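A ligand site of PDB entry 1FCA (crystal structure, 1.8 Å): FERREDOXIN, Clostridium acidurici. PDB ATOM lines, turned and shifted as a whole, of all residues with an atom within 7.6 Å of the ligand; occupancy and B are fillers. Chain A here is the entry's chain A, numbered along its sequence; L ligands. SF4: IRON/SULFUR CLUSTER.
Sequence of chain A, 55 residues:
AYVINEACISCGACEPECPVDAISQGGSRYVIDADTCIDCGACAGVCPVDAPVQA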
ATOM      1  N   VAL A   3      16.561   2.253 -30.782  1.00  0.00           N
ATOM      2  CA  VAL A   3      15.668   3.371 -30.977  1.00  0.00           C
ATOM      3  C   VAL A   3      14.290   2.800 -31.317  1.00  0.00           C
ATOM      4  O   VAL A   3      14.151   1.822 -32.073  1.00  0.00           O
ATOM      5  CB  VAL A   3      16.265   4.289 -32.112  1.00  0.00           C
ATOM      6  CG1 VAL A   3      16.350   3.534 -33.438  1.00  0.00           C
ATOM      7  CG2 VAL A   3      15.395   5.525 -32.275  1.00  0.00           C
ATOM      8  N   ILE A   4      13.247   3.386 -30.746  1.00  0.00           N
ATOM      9  CA  ILE A   4      11.891   2.968 -31.045  1.00  0.00           C
ATOM     10  C   ILE A   4      11.420   3.683 -32.299  1.00  0.00           C
ATOM     11  O   ILE A   4      11.411   4.908 -32.357  1.00  0.00           O
ATOM     12  CB  ILE A   4      11.013   3.307 -29.829  1.00  0.00           C
ATOM     13  CG1 ILE A   4      11.449   2.391 -28.679  1.00  0.00           C
ATOM     14  CG2 ILE A   4       9.540   3.079 -30.132  1.00  0.00           C
ATOM     15  CD1 ILE A   4      10.874   2.718 -27.293  1.00  0.00           C
ATOM     16  N   ASN A   5      11.057   2.907 -33.336  1.00  0.00           N
ATOM     17  CA  ASN A   5      10.680   3.537 -34.578  1.00  0.00           C
ATOM     18  C   ASN A   5       9.193   3.833 -34.660  1.00  0.00           C
ATOM     19  O   ASN A   5       8.488   3.717 -33.647  1.00  0.00           O
ATOM     20  CB  ASN A   5      11.181   2.636 -35.733  1.00  0.00           C
ATOM     21  CG  ASN A   5      10.597   1.263 -35.926  1.00  0.00           C
ATOM     22  OD1 ASN A   5      11.264   0.427 -36.550  1.00  0.00           O
ATOM     23  ND2 ASN A   5       9.407   0.918 -35.436  1.00  0.00           N
ATOM     24  N   ALA A   7       6.590   2.300 -35.859  1.00  0.00           N
ATOM     25  CA  ALA A   7       5.608   1.247 -35.702  1.00  0.00           C
ATOM     26  C   ALA A   7       5.067   1.210 -34.263  1.00  0.00           C
ATOM     27  O   ALA A   7       4.015   0.604 -34.036  1.00  0.00           O
ATOM     28  CB  ALA A   7       6.224  -0.101 -36.045  1.00  0.00           C
ATOM     29  N   CYS A   8       5.701   1.875 -33.277  1.00  0.00           N
ATOM     30  CA  CYS A   8       5.239   1.891 -31.883  1.00  0.00           C
ATOM     31  C   CYS A   8       3.776   2.267 -31.722  1.00  0.00           C
ATOM     32  O   CYS A   8       3.358   3.307 -32.241  1.00  0.00           O
ATOM     33  CB  CYS A   8       6.084   2.858 -31.078  1.00  0.00           C
ATOM     34  SG  CYS A   8       5.648   2.961 -29.326  1.00  0.00           S
ATOM     35  N   ILE A   9       2.980   1.436 -31.030  1.00  0.00           N
ATOM     36  CA  ILE A   9       1.566   1.742 -30.798  1.00  0.00           C
ATOM     37  C   ILE A   9       1.277   2.247 -29.393  1.00  0.00           C
ATOM     38  O   ILE A   9       0.115   2.368 -28.969  1.00  0.00           O
ATOM     39  CB  ILE A   9       0.699   0.484 -31.111  1.00  0.00           C
ATOM     40  CG1 ILE A   9       1.168  -0.740 -30.275  1.00  0.00           C
ATOM     41  CG2 ILE A   9       0.757   0.235 -32.603  1.00  0.00           C
ATOM     42  CD1 ILE A   9       0.311  -2.028 -30.398  1.00  0.00           C
ATOM     43  N   SER A  10       2.359   2.552 -28.639  1.00  0.00           N
ATOM     44  CA  SER A  10       2.312   3.107 -27.282  1.00  0.00           C
ATOM     45  C   SER A  10       1.550   2.262 -26.267  1.00  0.00           C
ATOM     46  O   SER A  10       0.825   2.754 -25.387  1.00  0.00           O
ATOM     47  CB  SER A  10       1.734   4.534 -27.316  1.00  0.00           C
ATOM     48  OG  SER A  10       2.607   5.366 -28.070  1.00  0.00           O
ATOM     49  N   CYS A  11       1.745   0.949 -26.375  1.00  0.00           N
ATOM     50  CA  CYS A  11       1.105  -0.001 -25.473  1.00  0.00           C
ATOM     51  C   CYS A  11       1.727   0.049 -24.069  1.00  0.00           C
ATOM     52  O   CYS A  11       1.109  -0.346 -23.069  1.00  0.00           O
ATOM     53  CB  CYS A  11       1.218  -1.393 -26.087  1.00  0.00           C
ATOM     54  SG  CYS A  11       2.813  -2.210 -25.941  1.00  0.00           S
ATOM     55  N   GLY A  12       2.972   0.533 -23.973  1.00  0.00           N
ATOM     56  CA  GLY A  12       3.665   0.679 -22.703  1.00  0.00           C
ATOM     57  C   GLY A  12       4.292  -0.593 -22.145  1.00  0.00           C
ATOM     58  O   GLY A  12       4.907  -0.536 -21.086  1.00  0.00           O
ATOM     59  N   ALA A  13       4.204  -1.741 -22.832  1.00  0.00           N
ATOM     60  CA  ALA A  13       4.697  -2.985 -22.246  1.00  0.00           C
ATOM     61  C   ALA A  13       6.217  -3.060 -22.074  1.00  0.00           C
ATOM     62  O   ALA A  13       6.686  -3.813 -21.203  1.00  0.00           O
ATOM     63  CB  ALA A  13       4.251  -4.162 -23.117  1.00  0.00           C
ATOM     64  N   CYS A  14       6.982  -2.271 -22.839  1.00  0.00           N
ATOM     65  CA  CYS A  14       8.426  -2.312 -22.713  1.00  0.00           C
ATOM     66  C   CYS A  14       8.979  -1.494 -21.564  1.00  0.00           C
ATOM     67  O   CYS A  14      10.053  -1.849 -21.049  1.00  0.00           O
ATOM     68  CB  CYS A  14       9.075  -1.811 -23.997  1.00  0.00           C
ATOM     69  SG  CYS A  14       8.465  -0.142 -24.344  1.00  0.00           S
ATOM     70  N   GLU A  15       8.268  -0.453 -21.134  1.00  0.00           N
ATOM     71  CA  GLU A  15       8.805   0.415 -20.093  1.00  0.00           C
ATOM     72  C   GLU A  15       9.249  -0.301 -18.805  1.00  0.00           C
ATOM     73  O   GLU A  15      10.427  -0.141 -18.474  1.00  0.00           O
ATOM     74  CB  GLU A  15       7.783   1.470 -19.775  1.00  0.00           C
ATOM     75  CG  GLU A  15       8.484   2.512 -18.966  1.00  0.00           C
ATOM     76  CD  GLU A  15       7.563   3.638 -18.545  1.00  0.00           C
ATOM     77  OE1 GLU A  15       6.529   3.898 -19.158  1.00  0.00           O
ATOM     78  OE2 GLU A  15       7.925   4.276 -17.568  1.00  0.00           O
ATOM     79  N   ILE A  23      13.652   3.630 -20.912  1.00  0.00           N
ATOM     80  CA  ILE A  23      12.468   3.932 -21.720  1.00  0.00           C
ATOM     81  C   ILE A  23      11.432   4.770 -20.977  1.00  0.00           C
ATOM     82  O   ILE A  23      11.135   4.536 -19.803  1.00  0.00           O
ATOM     83  CB  ILE A  23      11.787   2.592 -22.187  1.00  0.00           C
ATOM     84  CG1 ILE A  23      12.777   1.768 -22.998  1.00  0.00           C
ATOM     85  CG2 ILE A  23      10.541   2.893 -23.060  1.00  0.00           C
ATOM     86  CD1 ILE A  23      12.236   0.366 -23.352  1.00  0.00           C
ATOM     87  N   SER A  24      10.872   5.769 -21.661  1.00  0.00           N
ATOM     88  CA  SER A  24       9.780   6.557 -21.112  1.00  0.00           C
ATOM     89  C   SER A  24       8.747   6.853 -22.183  1.00  0.00           C
ATOM     90  O   SER A  24       8.971   6.676 -23.379  1.00  0.00           O
ATOM     91  CB  SER A  24      10.302   7.878 -20.526  1.00  0.00           C
ATOM     92  OG  SER A  24      10.930   8.665 -21.516  1.00  0.00           O
ATOM     93  N   GLN A  25       7.551   7.259 -21.726  1.00  0.00           N
ATOM     94  CA  GLN A  25       6.467   7.634 -22.610  1.00  0.00           C
ATOM     95  C   GLN A  25       6.765   8.988 -23.230  1.00  0.00           C
ATOM     96  O   GLN A  25       7.210   9.898 -22.547  1.00  0.00           O
ATOM     97  CB  GLN A  25       5.153   7.717 -21.825  1.00  0.00           C
ATOM     98  CG  GLN A  25       3.942   8.020 -22.700  1.00  0.00           C
ATOM     99  CD  GLN A  25       2.571   7.741 -22.072  1.00  0.00           C
ATOM    100  OE1 GLN A  25       2.067   6.616 -22.127  1.00  0.00           O
ATOM    101  NE2 GLN A  25       1.887   8.724 -21.476  1.00  0.00           N
ATOM    102  N   ARG A  29       5.062   8.436 -29.478  1.00  0.00           N
ATOM    103  CA  ARG A  29       5.727   7.110 -29.268  1.00  0.00           C
ATOM    104  C   ARG A  29       6.614   7.076 -28.044  1.00  0.00           C
ATOM    105  O   ARG A  29       6.972   8.120 -27.500  1.00  0.00           O
ATOM    106  CB  ARG A  29       6.603   6.623 -30.478  1.00  0.00           C
ATOM    107  CG  ARG A  29       7.636   7.545 -31.101  1.00  0.00           C
ATOM    108  CD  ARG A  29       8.434   6.886 -32.254  1.00  0.00           C
ATOM    109  NE  ARG A  29       8.674   7.839 -33.336  1.00  0.00           N
ATOM    110  CZ  ARG A  29       9.824   7.971 -34.014  1.00  0.00           C
ATOM    111  NH1 ARG A  29      10.942   7.305 -33.744  1.00  0.00           N
ATOM    112  NH2 ARG A  29       9.864   8.872 -35.005  1.00  0.00           N
ATOM    113  N   TYR A  30       6.948   5.879 -27.554  1.00  0.00           N
ATOM    114  CA  TYR A  30       7.869   5.748 -26.437  1.00  0.00           C
ATOM    115  C   TYR A  30       9.287   6.073 -26.928  1.00  0.00           C
ATOM    116  O   TYR A  30       9.570   5.972 -28.116  1.00  0.00           O
ATOM    117  CB  TYR A  30       7.765   4.312 -25.862  1.00  0.00           C
ATOM    118  CG  TYR A  30       6.600   4.205 -24.877  1.00  0.00           C
ATOM    119  CD1 TYR A  30       5.296   4.458 -25.284  1.00  0.00           C
ATOM    120  CD2 TYR A  30       6.859   3.870 -23.548  1.00  0.00           C
ATOM    121  CE1 TYR A  30       4.266   4.412 -24.378  1.00  0.00           C
ATOM    122  CE2 TYR A  30       5.824   3.816 -22.637  1.00  0.00           C
ATOM    123  CZ  TYR A  30       4.546   4.092 -23.067  1.00  0.00           C
ATOM    124  OH  TYR A  30       3.525   4.090 -22.148  1.00  0.00           O
ATOM    125  N   VAL A  31      10.177   6.467 -26.015  1.00  0.00           N
ATOM    126  CA  VAL A  31      11.526   6.924 -26.362  1.00  0.00           C
ATOM    127  C   VAL A  31      12.592   6.262 -25.507  1.00  0.00           C
ATOM    128  O   VAL A  31      12.424   6.109 -24.305  1.00  0.00           O
ATOM    129  CB  VAL A  31      11.879   8.427 -26.113  1.00  0.00           C
ATOM    130  CG1 VAL A  31      12.421   8.961 -27.417  1.00  0.00           C
ATOM    131  CG2 VAL A  31      10.765   9.189 -25.479  1.00  0.00           C
ATOM    132  N   ILE A  32      13.744   5.986 -26.126  1.00  0.00           N
ATOM    133  CA  ILE A  32      14.881   5.404 -25.428  1.00  0.00           C
ATOM    134  C   ILE A  32      15.913   6.494 -25.152  1.00  0.00           C
ATOM    135  O   ILE A  32      16.241   7.296 -26.016  1.00  0.00           O
ATOM    136  CB  ILE A  32      15.501   4.301 -26.307  1.00  0.00           C
ATOM    137  CG1 ILE A  32      14.501   3.149 -26.356  1.00  0.00           C
ATOM    138  CG2 ILE A  32      16.896   3.841 -25.782  1.00  0.00           C
ATOM    139  CD1 ILE A  32      14.901   1.999 -27.283  1.00  0.00           C
ATOM    140  N   CYS A  43      13.508  -4.859 -24.691  1.00  0.00           N
ATOM    141  CA  CYS A  43      12.363  -4.094 -25.170  1.00  0.00           C
ATOM    142  C   CYS A  43      11.820  -4.623 -26.478  1.00  0.00           C
ATOM    143  O   CYS A  43      10.608  -4.633 -26.644  1.00  0.00           O
ATOM    144  CB  CYS A  43      12.720  -2.620 -25.387  1.00  0.00           C
ATOM    145  SG  CYS A  43      14.266  -2.396 -26.306  1.00  0.00           S
ATOM    146  N   ALA A  44      12.668  -5.040 -27.429  1.00  0.00           N
ATOM    147  CA  ALA A  44      12.161  -5.604 -28.671  1.00  0.00           C
ATOM    148  C   ALA A  44      11.488  -6.960 -28.457  1.00  0.00           C
ATOM    149  O   ALA A  44      10.505  -7.260 -29.124  1.00  0.00           O
ATOM    150  CB  ALA A  44      13.270  -5.815 -29.689  1.00  0.00           C
ATOM    151  N   GLY A  45      11.996  -7.753 -27.484  1.00  0.00           N
ATOM    152  CA  GLY A  45      11.434  -9.056 -27.121  1.00  0.00           C
ATOM    153  C   GLY A  45      10.024  -8.971 -26.555  1.00  0.00           C
ATOM    154  O   GLY A  45       9.260  -9.928 -26.689  1.00  0.00           O
ATOM    155  N   VAL A  46       9.645  -7.893 -25.895  1.00  0.00           N
ATOM    156  CA  VAL A  46       8.266  -7.762 -25.412  1.00  0.00           C
ATOM    157  C   VAL A  46       7.414  -6.815 -26.267  1.00  0.00           C
ATOM    158  O   VAL A  46       6.258  -6.528 -25.943  1.00  0.00           O
ATOM    159  CB  VAL A  46       8.257  -7.282 -23.922  1.00  0.00           C
ATOM    160  CG1 VAL A  46       8.925  -8.371 -23.095  1.00  0.00           C
ATOM    161  CG2 VAL A  46       8.939  -5.925 -23.755  1.00  0.00           C
ATOM    162  N   CYS A  47       7.953  -6.326 -27.395  1.00  0.00           N
ATOM    163  CA  CYS A  47       7.197  -5.445 -28.268  1.00  0.00           C
ATOM    164  C   CYS A  47       6.359  -6.211 -29.283  1.00  0.00           C
ATOM    165  O   CYS A  47       6.919  -6.944 -30.092  1.00  0.00           O
ATOM    166  CB  CYS A  47       8.125  -4.510 -29.041  1.00  0.00           C
ATOM    167  SG  CYS A  47       7.075  -3.369 -29.977  1.00  0.00           S
ATOM    168  N   PRO A  48       5.022  -6.099 -29.297  1.00  0.00           N
ATOM    169  CA  PRO A  48       4.159  -6.834 -30.231  1.00  0.00           C
ATOM    170  C   PRO A  48       4.364  -6.467 -31.695  1.00  0.00           C
ATOM    171  O   PRO A  48       4.142  -7.296 -32.582  1.00  0.00           O
ATOM    172  CB  PRO A  48       2.761  -6.560 -29.723  1.00  0.00           C
ATOM    173  CG  PRO A  48       2.881  -5.164 -29.092  1.00  0.00           C
ATOM    174  CD  PRO A  48       4.241  -5.262 -28.399  1.00  0.00           C
ATOM    175  N   VAL A  49       4.791  -5.210 -31.956  1.00  0.00           N
ATOM    176  CA  VAL A  49       5.019  -4.729 -33.309  1.00  0.00           C
ATOM    177  C   VAL A  49       6.501  -4.626 -33.671  1.00  0.00           C
ATOM    178  O   VAL A  49       6.845  -4.090 -34.724  1.00  0.00           O
ATOM    179  CB  VAL A  49       4.341  -3.353 -33.502  1.00  0.00           C
ATOM    180  CG1 VAL A  49       2.839  -3.547 -33.437  1.00  0.00           C
ATOM    181  CG2 VAL A  49       4.795  -2.342 -32.437  1.00  0.00           C
ATOM    182  N   ASP A  50       7.389  -5.114 -32.783  1.00  0.00           N
ATOM    183  CA  ASP A  50       8.845  -5.085 -32.933  1.00  0.00           C
ATOM    184  C   ASP A  50       9.369  -3.694 -33.327  1.00  0.00           C
ATOM    185  O   ASP A  50      10.148  -3.547 -34.261  1.00  0.00           O
ATOM    186  CB  ASP A  50       9.205  -6.180 -33.963  1.00  0.00           C
ATOM    187  CG  ASP A  50      10.640  -6.671 -33.894  1.00  0.00           C
ATOM    188  OD1 ASP A  50      11.157  -6.960 -32.806  1.00  0.00           O
ATOM    189  OD2 ASP A  50      11.235  -6.793 -34.958  1.00  0.00           O
ATOM    190  N   ALA A  51       8.919  -2.648 -32.644  1.00  0.00           N
ATOM    191  CA  ALA A  51       9.383  -1.291 -32.947  1.00  0.00           C
ATOM    192  C   ALA A  51      10.805  -0.931 -32.501  1.00  0.00           C
ATOM    193  O   ALA A  51      11.440  -0.156 -33.236  1.00  0.00           O
ATOM    194  CB  ALA A  51       8.418  -0.279 -32.347  1.00  0.00           C
ATOM    195  N   PRO A  52      11.385  -1.389 -31.353  1.00  0.00           N
ATOM    196  CA  PRO A  52      12.769  -1.119 -30.956  1.00  0.00           C
ATOM    197  C   PRO A  52      13.752  -1.803 -31.894  1.00  0.00           C
ATOM    198  O   PRO A  52      13.707  -3.029 -32.038  1.00  0.00           O
ATOM    199  CB  PRO A  52      12.886  -1.650 -29.528  1.00  0.00           C
ATOM    200  CG  PRO A  52      11.446  -1.658 -29.044  1.00  0.00           C
ATOM    201  CD  PRO A  52      10.708  -2.139 -30.277  1.00  0.00           C
HETATM  202 FE1  SF4 L   1       5.969   0.907 -28.324  1.00  0.00          FE
HETATM  203 FE2  SF4 L   1       4.591  -1.041 -26.875  1.00  0.00          FE
HETATM  204 FE3  SF4 L   1       7.213  -0.331 -26.267  1.00  0.00          FE
HETATM  205 FE4  SF4 L   1       6.705  -1.699 -28.462  1.00  0.00          FE
HETATM  206  S1  SF4 L   1       6.329  -2.478 -26.345  1.00  0.00           S
HETATM  207  S2  SF4 L   1       8.151   0.079 -28.331  1.00  0.00           S
HETATM  208  S3  SF4 L   1       4.656  -0.826 -29.152  1.00  0.00           S
HETATM  209  S4  SF4 L   1       5.296   1.020 -26.123  1.00  0.00           S
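N of Gly 12 lies close to S4 of the ligand (3.2 Å).
S4 of the ligand sits close to N of Cys 11.
The side-chain sulfur (SG) of Cys 14 binds an iron atom (FE3) of the ligand.
The backbone NH (N) of Ile 9 sits close to a sulfur (S3) of the ligand, at 3.4 Å.
The side-chain sulfur (SG) of Cys 11 binds an iron atom (FE2) of the ligand (2.3 Å).
N of Cys 14 sits close to S1 of the ligand (3.6 Å).
The side-chain sulfur of Cys 8 is bound to an iron atom (FE1) of the ligand.
SG of Cys 47 binds FE4 of the ligand, 2.3 Å away.
N of Ser 10 sits close to SG of Cys 8 (3.4 Å).
The backbone NH of Ala 51 lies close to the side-chain sulfur of Cys 47.
The backbone NH (N) of Val 49 sits close to the side-chain sulfur (SG) of Cys 47, 3.5 Å away.
SG of Cys 11 lies close to N of Ala 13 (3.4 Å).
The backbone carbonyl oxygen (O) of Ile 4 is in hydrogen-bond range of the guanidinium group (NH1) of Arg 29, 2.8 Å away.
OE1 of Gln 25 lies within hydrogen-bond range of OH of Tyr 30 (2.9 Å).
The backbone NH (N) of Tyr 30 lies close to the side-chain sulfur (SG) of Cys 8.
SG of Cys 47 lies close to N of Asp 50 (3.3 Å).
Ile 4 touches the ligand.
Ser 10 touches the ligand (CA to S4, 3.8 Å).
CD1 of Tyr 30 touches S4 of the ligand, 3.5 Å away.
CG2 of Val 49 touches S3 of the ligand, at 3.6 Å.
Pro 52 touches the ligand.
Hydrophobic or aromatic side chains that line the ligand: Ile 4, Ile 9, Tyr 30, Val 49 and Pro 52.
The nearest printed residue that does not touch the ligand is Ala 51 (4.04 Å).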
